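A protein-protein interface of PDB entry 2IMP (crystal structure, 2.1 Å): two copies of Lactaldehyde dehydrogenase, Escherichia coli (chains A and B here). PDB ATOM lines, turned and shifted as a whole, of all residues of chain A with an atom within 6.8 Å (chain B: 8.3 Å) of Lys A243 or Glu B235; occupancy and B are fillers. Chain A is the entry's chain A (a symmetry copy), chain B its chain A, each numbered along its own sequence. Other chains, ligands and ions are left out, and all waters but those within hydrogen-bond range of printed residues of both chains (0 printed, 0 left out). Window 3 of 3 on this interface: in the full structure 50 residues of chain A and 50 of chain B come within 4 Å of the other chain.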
ATOM      1  N   GLN A 214     -27.730  19.803  33.334  1.00  0.00           N
ATOM      2  CA  GLN A 214     -26.524  19.031  33.596  1.00  0.00           C
ATOM      3  C   GLN A 214     -26.806  17.562  33.954  1.00  0.00           C
ATOM      4  O   GLN A 214     -26.050  16.669  33.563  1.00  0.00           O
ATOM      5  CB  GLN A 214     -25.701  19.698  34.697  1.00  0.00           C
ATOM      6  CG  GLN A 214     -24.824  20.833  34.185  1.00  0.00           C
ATOM      7  CD  GLN A 214     -23.678  20.337  33.310  1.00  0.00           C
ATOM      8  OE1 GLN A 214     -22.799  19.619  33.779  1.00  0.00           O
ATOM      9  NE2 GLN A 214     -23.688  20.718  32.034  1.00  0.00           N
ATOM     10  N   GLY A 218     -25.223  14.368  32.226  1.00  0.00           N
ATOM     11  CA  GLY A 218     -24.321  13.533  32.998  1.00  0.00           C
ATOM     12  C   GLY A 218     -24.824  12.228  33.580  1.00  0.00           C
ATOM     13  O   GLY A 218     -24.031  11.445  34.097  1.00  0.00           O
ATOM     14  N   MET A 238     -21.246  18.798  26.587  1.00  0.00           N
ATOM     15  CA  MET A 238     -20.350  17.783  26.066  1.00  0.00           C
ATOM     16  C   MET A 238     -19.283  17.366  27.087  1.00  0.00           C
ATOM     17  O   MET A 238     -18.977  16.186  27.222  1.00  0.00           O
ATOM     18  CB  MET A 238     -19.675  18.269  24.782  1.00  0.00           C
ATOM     19  CG  MET A 238     -18.832  17.205  24.092  1.00  0.00           C
ATOM     20  SD  MET A 238     -18.236  17.748  22.476  1.00  0.00           S
ATOM     21  CE  MET A 238     -17.103  16.396  22.076  1.00  0.00           C
ATOM     22  N   ALA A 239     -18.728  18.347  27.797  1.00  0.00           N
ATOM     23  CA  ALA A 239     -17.735  18.039  28.809  1.00  0.00           C
ATOM     24  C   ALA A 239     -18.316  17.079  29.868  1.00  0.00           C
ATOM     25  O   ALA A 239     -17.666  16.121  30.287  1.00  0.00           O
ATOM     26  CB  ALA A 239     -17.255  19.326  29.477  1.00  0.00           C
ATOM     27  N   THR A 240     -19.554  17.346  30.270  1.00  0.00           N
ATOM     28  CA  THR A 240     -20.218  16.505  31.254  1.00  0.00           C
ATOM     29  C   THR A 240     -20.554  15.114  30.700  1.00  0.00           C
ATOM     30  O   THR A 240     -20.402  14.106  31.393  1.00  0.00           O
ATOM     31  CB  THR A 240     -21.490  17.195  31.774  1.00  0.00           C
ATOM     32  OG1 THR A 240     -21.109  18.376  32.491  1.00  0.00           O
ATOM     33  CG2 THR A 240     -22.271  16.278  32.698  1.00  0.00           C
ATOM     34  N   ALA A 241     -20.995  15.074  29.446  1.00  0.00           N
ATOM     35  CA  ALA A 241     -21.301  13.803  28.803  1.00  0.00           C
ATOM     36  C   ALA A 241     -20.055  12.896  28.722  1.00  0.00           C
ATOM     37  O   ALA A 241     -20.153  11.672  28.794  1.00  0.00           O
ATOM     38  CB  ALA A 241     -21.863  14.047  27.401  1.00  0.00           C
ATOM     39  N   ALA A 242     -18.892  13.533  28.596  1.00  0.00           N
ATOM     40  CA  ALA A 242     -17.623  12.832  28.514  1.00  0.00           C
ATOM     41  C   ALA A 242     -17.380  11.854  29.678  1.00  0.00           C
ATOM     42  O   ALA A 242     -16.808  10.783  29.485  1.00  0.00           O
ATOM     43  CB  ALA A 242     -16.476  13.845  28.434  1.00  0.00           C
ATOM     44  N   LYS A 243     -17.819  12.237  30.875  1.00  0.00           N
ATOM     45  CA  LYS A 243     -17.653  11.396  32.056  1.00  0.00           C
ATOM     46  C   LYS A 243     -18.172   9.950  31.875  1.00  0.00           C
ATOM     47  O   LYS A 243     -17.633   9.007  32.446  1.00  0.00           O
ATOM     48  CB  LYS A 243     -18.350  12.040  33.261  1.00  0.00           C
ATOM     49  CG  LYS A 243     -17.699  13.342  33.723  1.00  0.00           C
ATOM     50  CD  LYS A 243     -18.391  13.908  34.961  1.00  0.00           C
ATOM     51  CE  LYS A 243     -17.590  15.056  35.577  1.00  0.00           C
ATOM     52  NZ  LYS A 243     -17.382  16.197  34.637  1.00  0.00           N
ATOM     53  N   ASN A 244     -19.228   9.802  31.088  1.00  0.00           N
ATOM     54  CA  ASN A 244     -19.796   8.490  30.831  1.00  0.00           C
ATOM     55  C   ASN A 244     -19.712   8.080  29.353  1.00  0.00           C
ATOM     56  O   ASN A 244     -20.355   7.118  28.925  1.00  0.00           O
ATOM     57  CB  ASN A 244     -21.259   8.461  31.283  1.00  0.00           C
ATOM     58  CG  ASN A 244     -21.420   8.796  32.756  1.00  0.00           C
ATOM     59  OD1 ASN A 244     -20.884   8.111  33.623  1.00  0.00           O
ATOM     60  ND2 ASN A 244     -22.167   9.854  33.043  1.00  0.00           N
ATOM     61  N   ILE A 245     -18.897   8.801  28.592  1.00  0.00           N
ATOM     62  CA  ILE A 245     -18.771   8.529  27.168  1.00  0.00           C
ATOM     63  C   ILE A 245     -20.165   8.567  26.483  1.00  0.00           C
ATOM     64  O   ILE A 245     -20.479   7.776  25.590  1.00  0.00           O
ATOM     65  CB  ILE A 245     -18.121   7.150  26.912  1.00  0.00           C
ATOM     66  CG1 ILE A 245     -16.917   6.958  27.842  1.00  0.00           C
ATOM     67  CG2 ILE A 245     -17.657   7.052  25.445  1.00  0.00           C
ATOM     68  CD1 ILE A 245     -15.807   7.995  27.639  1.00  0.00           C
ATOM     69  N   THR A 246     -20.992   9.495  26.951  1.00  0.00           N
ATOM     70  CA  THR A 246     -22.335   9.662  26.420  1.00  0.00           C
ATOM     71  C   THR A 246     -22.368  10.381  25.061  1.00  0.00           C
ATOM     72  O   THR A 246     -21.758  11.435  24.881  1.00  0.00           O
ATOM     73  CB  THR A 246     -23.229  10.429  27.428  1.00  0.00           C
ATOM     74  OG1 THR A 246     -23.333   9.667  28.639  1.00  0.00           O
ATOM     75  CG2 THR A 246     -24.625  10.653  26.861  1.00  0.00           C
ATOM     76  N   GLN B 214      -3.218  15.172  24.521  1.00  0.00           N
ATOM     77  CA  GLN B 214      -4.157  16.234  24.850  1.00  0.00           C
ATOM     78  C   GLN B 214      -4.184  17.368  23.810  1.00  0.00           C
ATOM     79  O   GLN B 214      -5.245  17.928  23.526  1.00  0.00           O
ATOM     80  CB  GLN B 214      -3.854  16.795  26.238  1.00  0.00           C
ATOM     81  CG  GLN B 214      -4.453  15.961  27.364  1.00  0.00           C
ATOM     82  CD  GLN B 214      -5.973  16.049  27.409  1.00  0.00           C
ATOM     83  OE1 GLN B 214      -6.531  17.116  27.649  1.00  0.00           O
ATOM     84  NE2 GLN B 214      -6.647  14.923  27.175  1.00  0.00           N
ATOM     85  N   MET B 227      -9.563   8.012  18.737  1.00  0.00           N
ATOM     86  CA  MET B 227      -8.735   7.291  19.680  1.00  0.00           C
ATOM     87  C   MET B 227      -9.250   5.910  20.099  1.00  0.00           C
ATOM     88  O   MET B 227     -10.453   5.680  20.225  1.00  0.00           O
ATOM     89  CB  MET B 227      -8.514   8.157  20.932  1.00  0.00           C
ATOM     90  CG  MET B 227      -7.837   7.445  22.102  1.00  0.00           C
ATOM     91  SD  MET B 227      -8.996   6.664  23.257  1.00  0.00           S
ATOM     92  CE  MET B 227      -7.865   5.992  24.478  1.00  0.00           C
ATOM     93  N   SER B 230      -8.040   2.829  26.606  1.00  0.00           N
ATOM     94  CA  SER B 230      -8.770   2.791  27.878  1.00  0.00           C
ATOM     95  C   SER B 230      -9.905   3.814  28.009  1.00  0.00           C
ATOM     96  O   SER B 230      -9.824   4.918  27.469  1.00  0.00           O
ATOM     97  CB  SER B 230      -7.813   2.993  29.059  1.00  0.00           C
ATOM     98  OG  SER B 230      -7.428   4.355  29.178  1.00  0.00           O
ATOM     99  N   VAL B 231     -10.949   3.432  28.737  1.00  0.00           N
ATOM    100  CA  VAL B 231     -12.081   4.316  28.952  1.00  0.00           C
ATOM    101  C   VAL B 231     -11.683   5.602  29.711  1.00  0.00           C
ATOM    102  O   VAL B 231     -12.261   6.668  29.501  1.00  0.00           O
ATOM    103  CB  VAL B 231     -13.217   3.591  29.725  1.00  0.00           C
ATOM    104  CG1 VAL B 231     -12.750   3.210  31.115  1.00  0.00           C
ATOM    105  CG2 VAL B 231     -14.441   4.484  29.803  1.00  0.00           C
ATOM    106  N   SER B 232     -10.683   5.480  30.582  1.00  0.00           N
ATOM    107  CA  SER B 232     -10.198   6.624  31.340  1.00  0.00           C
ATOM    108  C   SER B 232      -9.587   7.708  30.427  1.00  0.00           C
ATOM    109  O   SER B 232      -9.854   8.904  30.583  1.00  0.00           O
ATOM    110  CB  SER B 232      -9.157   6.172  32.368  1.00  0.00           C
ATOM    111  OG  SER B 232      -8.667   7.280  33.101  1.00  0.00           O
ATOM    112  N   ALA B 233      -8.766   7.268  29.480  1.00  0.00           N
ATOM    113  CA  ALA B 233      -8.162   8.189  28.532  1.00  0.00           C
ATOM    114  C   ALA B 233      -9.212   8.779  27.568  1.00  0.00           C
ATOM    115  O   ALA B 233      -9.154   9.958  27.215  1.00  0.00           O
ATOM    116  CB  ALA B 233      -7.080   7.482  27.742  1.00  0.00           C
ATOM    117  N   GLY B 234     -10.165   7.937  27.167  1.00  0.00           N
ATOM    118  CA  GLY B 234     -11.225   8.376  26.279  1.00  0.00           C
ATOM    119  C   GLY B 234     -12.028   9.493  26.921  1.00  0.00           C
ATOM    120  O   GLY B 234     -12.441  10.445  26.247  1.00  0.00           O
ATOM    121  N   GLU B 235     -12.264   9.376  28.226  1.00  0.00           N
ATOM    122  CA  GLU B 235     -13.000  10.405  28.955  1.00  0.00           C
ATOM    123  C   GLU B 235     -12.266  11.761  28.945  1.00  0.00           C
ATOM    124  O   GLU B 235     -12.869  12.816  28.745  1.00  0.00           O
ATOM    125  CB  GLU B 235     -13.207   9.989  30.411  1.00  0.00           C
ATOM    126  CG  GLU B 235     -14.132   8.807  30.630  1.00  0.00           C
ATOM    127  CD  GLU B 235     -14.136   8.353  32.088  1.00  0.00           C
ATOM    128  OE1 GLU B 235     -14.216   9.232  32.979  1.00  0.00           O
ATOM    129  OE2 GLU B 235     -14.062   7.127  32.340  1.00  0.00           O
ATOM    130  N   LYS B 236     -10.960  11.705  29.178  1.00  0.00           N
ATOM    131  CA  LYS B 236     -10.149  12.905  29.187  1.00  0.00           C
ATOM    132  C   LYS B 236     -10.063  13.539  27.797  1.00  0.00           C
ATOM    133  O   LYS B 236     -10.039  14.759  27.656  1.00  0.00           O
ATOM    134  CB  LYS B 236      -8.748  12.582  29.708  1.00  0.00           C
ATOM    135  CG  LYS B 236      -8.737  12.069  31.153  1.00  0.00           C
ATOM    136  CD  LYS B 236      -7.324  11.774  31.631  1.00  0.00           C
ATOM    137  CE  LYS B 236      -7.318  11.247  33.056  1.00  0.00           C
ATOM    138  NZ  LYS B 236      -8.009   9.931  33.147  1.00  0.00           N
ATOM    139  N   ILE B 237     -10.018  12.683  26.782  1.00  0.00           N
ATOM    140  CA  ILE B 237      -9.969  13.135  25.401  1.00  0.00           C
ATOM    141  C   ILE B 237     -11.262  13.859  24.996  1.00  0.00           C
ATOM    142  O   ILE B 237     -11.226  14.947  24.422  1.00  0.00           O
ATOM    143  CB  ILE B 237      -9.735  11.948  24.438  1.00  0.00           C
ATOM    144  CG1 ILE B 237      -8.278  11.497  24.539  1.00  0.00           C
ATOM    145  CG2 ILE B 237     -10.067  12.350  23.002  1.00  0.00           C
ATOM    146  CD1 ILE B 237      -7.977  10.198  23.849  1.00  0.00           C
ATOM    147  N   MET B 238     -12.396  13.244  25.317  1.00  0.00           N
ATOM    148  CA  MET B 238     -13.677  13.841  24.987  1.00  0.00           C
ATOM    149  C   MET B 238     -13.931  15.142  25.760  1.00  0.00           C
ATOM    150  O   MET B 238     -14.430  16.112  25.200  1.00  0.00           O
ATOM    151  CB  MET B 238     -14.814  12.852  25.251  1.00  0.00           C
ATOM    152  CG  MET B 238     -16.177  13.349  24.789  1.00  0.00           C
ATOM    153  SD  MET B 238     -17.449  12.072  24.917  1.00  0.00           S
ATOM    154  CE  MET B 238     -18.928  13.047  24.552  1.00  0.00           C
ATOM    155  N   ALA B 239     -13.584  15.144  27.046  1.00  0.00           N
ATOM    156  CA  ALA B 239     -13.757  16.343  27.844  1.00  0.00           C
ATOM    157  C   ALA B 239     -12.975  17.523  27.231  1.00  0.00           C
ATOM    158  O   ALA B 239     -13.473  18.646  27.146  1.00  0.00           O
ATOM    159  CB  ALA B 239     -13.288  16.091  29.276  1.00  0.00           C
ATOM    160  N   THR B 240     -11.753  17.238  26.792  1.00  0.00           N
ATOM    161  CA  THR B 240     -10.921  18.262  26.180  1.00  0.00           C
ATOM    162  C   THR B 240     -11.455  18.706  24.812  1.00  0.00           C
ATOM    163  O   THR B 240     -11.442  19.894  24.485  1.00  0.00           O
ATOM    164  CB  THR B 240      -9.471  17.767  26.053  1.00  0.00           C
ATOM    165  OG1 THR B 240      -8.932  17.586  27.369  1.00  0.00           O
ATOM    166  CG2 THR B 240      -8.616  18.764  25.292  1.00  0.00           C
ATOM    167  N   ALA B 241     -11.936  17.743  24.030  1.00  0.00           N
ATOM    168  CA  ALA B 241     -12.510  18.056  22.728  1.00  0.00           C
ATOM    169  C   ALA B 241     -13.733  18.989  22.860  1.00  0.00           C
ATOM    170  O   ALA B 241     -13.995  19.820  21.993  1.00  0.00           O
ATOM    171  CB  ALA B 241     -12.908  16.767  22.008  1.00  0.00           C
ATOM    172  N   ALA B 242     -14.450  18.837  23.972  1.00  0.00           N
ATOM    173  CA  ALA B 242     -15.627  19.638  24.257  1.00  0.00           C
ATOM    174  C   ALA B 242     -15.374  21.155  24.188  1.00  0.00           C
ATOM    175  O   ALA B 242     -16.235  21.912  23.743  1.00  0.00           O
ATOM    176  CB  ALA B 242     -16.187  19.264  25.633  1.00  0.00           C
ATOM    177  N   VAL B 248     -15.599  13.579  18.172  1.00  0.00           N
ATOM    178  CA  VAL B 248     -14.789  12.489  18.683  1.00  0.00           C
ATOM    179  C   VAL B 248     -15.203  11.111  18.136  1.00  0.00           C
ATOM    180  O   VAL B 248     -16.375  10.850  17.872  1.00  0.00           O
ATOM    181  CB  VAL B 248     -14.802  12.398  20.244  1.00  0.00           C
ATOM    182  CG1 VAL B 248     -14.412  13.741  20.860  1.00  0.00           C
ATOM    183  CG2 VAL B 248     -16.163  11.924  20.734  1.00  0.00           C
ATOM    184  N   LEU B 250     -14.337   7.311  19.329  1.00  0.00           N
ATOM    185  CA  LEU B 250     -13.691   6.495  20.342  1.00  0.00           C
ATOM    186  C   LEU B 250     -14.078   5.015  20.409  1.00  0.00           C
ATOM    187  O   LEU B 250     -15.231   4.634  20.206  1.00  0.00           O
ATOM    188  CB  LEU B 250     -13.944   7.104  21.730  1.00  0.00           C
ATOM    189  CG  LEU B 250     -13.741   8.612  21.919  1.00  0.00           C
ATOM    190  CD1 LEU B 250     -14.388   9.052  23.229  1.00  0.00           C
ATOM    191  CD2 LEU B 250     -12.255   8.941  21.899  1.00  0.00           C
ATOM    192  N   LEU B 252     -13.230   2.205  23.280  1.00  0.00           N
ATOM    193  CA  LEU B 252     -12.633   1.996  24.590  1.00  0.00           C
ATOM    194  C   LEU B 252     -12.692   0.569  25.197  1.00  0.00           C
ATOM    195  O   LEU B 252     -12.810   0.413  26.408  1.00  0.00           O
ATOM    196  CB  LEU B 252     -13.251   3.024  25.549  1.00  0.00           C
ATOM    197  CG  LEU B 252     -13.335   4.426  24.910  1.00  0.00           C
ATOM    198  CD1 LEU B 252     -14.153   5.380  25.782  1.00  0.00           C
ATOM    199  CD2 LEU B 252     -11.920   4.973  24.685  1.00  0.00           C
ATOM    200  N   TYR B 409     -19.940  -1.719  29.357  1.00  0.00           N
ATOM    201  CA  TYR B 409     -19.405  -1.879  28.020  1.00  0.00           C
ATOM    202  C   TYR B 409     -20.319  -2.701  27.098  1.00  0.00           C
ATOM    203  O   TYR B 409     -21.002  -3.622  27.550  1.00  0.00           O
ATOM    204  CB  TYR B 409     -18.015  -2.503  28.092  1.00  0.00           C
ATOM    205  CG  TYR B 409     -17.069  -1.713  28.963  1.00  0.00           C
ATOM    206  CD1 TYR B 409     -16.988  -1.952  30.335  1.00  0.00           C
ATOM    207  CD2 TYR B 409     -16.303  -0.678  28.427  1.00  0.00           C
ATOM    208  CE1 TYR B 409     -16.167  -1.178  31.154  1.00  0.00           C
ATOM    209  CE2 TYR B 409     -15.482   0.104  29.236  1.00  0.00           C
ATOM    210  CZ  TYR B 409     -15.419  -0.149  30.596  1.00  0.00           C
ATOM    211  OH  TYR B 409     -14.623   0.635  31.400  1.00  0.00           O
ATOM    212  N   LYS B 454     -20.283   2.618  27.267  1.00  0.00           N
ATOM    213  CA  LYS B 454     -18.940   3.174  27.408  1.00  0.00           C
ATOM    214  C   LYS B 454     -17.872   2.608  26.448  1.00  0.00           C
ATOM    215  O   LYS B 454     -16.730   3.061  26.452  1.00  0.00           O
ATOM    216  CB  LYS B 454     -18.453   3.045  28.857  1.00  0.00           C
ATOM    217  CG  LYS B 454     -19.251   3.882  29.842  1.00  0.00           C
ATOM    218  CD  LYS B 454     -18.597   3.914  31.217  1.00  0.00           C
ATOM    219  CE  LYS B 454     -19.427   4.734  32.197  1.00  0.00           C
ATOM    220  NZ  LYS B 454     -18.776   4.854  33.536  1.00  0.00           N
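The backbone NH (N) of Thr A246 is in hydrogen-bond range of the backbone carbonyl oxygen (O) of Ala A241, 3.0 Å away. O of Gly A218 lies within hydrogen-bond range of ND2 of Asn A244.
Of the 20 printed residues of chain B, 7 touch a printed residue of chain A. Along chain B the printed residues that touch a printed residue of chain A span positions 235 to 454. Printed residues of chain A that touch a printed residue of chain B: Met A238, Ala A239, Ala A242, Lys A243, Asn A244, Ile A245 and Thr A246. Among the printed residues, 11 pairs touch across the chains.
Ala A242 touches just these residues of chain B: Glu B235 (3.5 Å), Met B238 (3.7 Å) and Ala B239 (3.5 Å). Lys A243 touches just one residue of chain B: Glu B235. Of the printed residues of chain B, Thr A246 touches Met B238 (3.3 Å). Glu B235 touches just these residues of chain A: Ala A242 (3.5 Å), Lys A243 (3.5 Å) and Ile A245 (3.5 Å). Of the printed residues of chain A, Val B248 touches Met A238.
The backbone carbonyl oxygen of Lys A243 lies close to the side-chain carboxylate of Glu B235 (3.5 Å).
SD of Met A238 touches CA of Ala B242, at 3.7 Å. CE of Met A238 touches CG1 of Val B248, 3.97 Å away. Ala B242 touches Ala A239 (CB to N, 3.5 Å). CG of Glu B235 touches O of Ala A242, at 3.5 Å. CA of Ala A242 touches SD of Met B238, 3.7 Å away. Ala A242 touches Ala B239 (CB to N, 3.5 Å). CG of Lys B454 touches O of Asn A244, 3.5 Å away. Ile A245 touches Glu B235. Ile A245 touches Leu B252. O of Thr A246 touches CE of Met B238 (3.3 Å).
Met A238 touches Ala B242, and with the chains exchanged Ala A242 touches Met B238. Ala A239 touches Ala B242, and with the chains exchanged Ala A242 touches Ala B239. Positions printed for both chains: 214, 238, 239, 240, 241 and 242.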
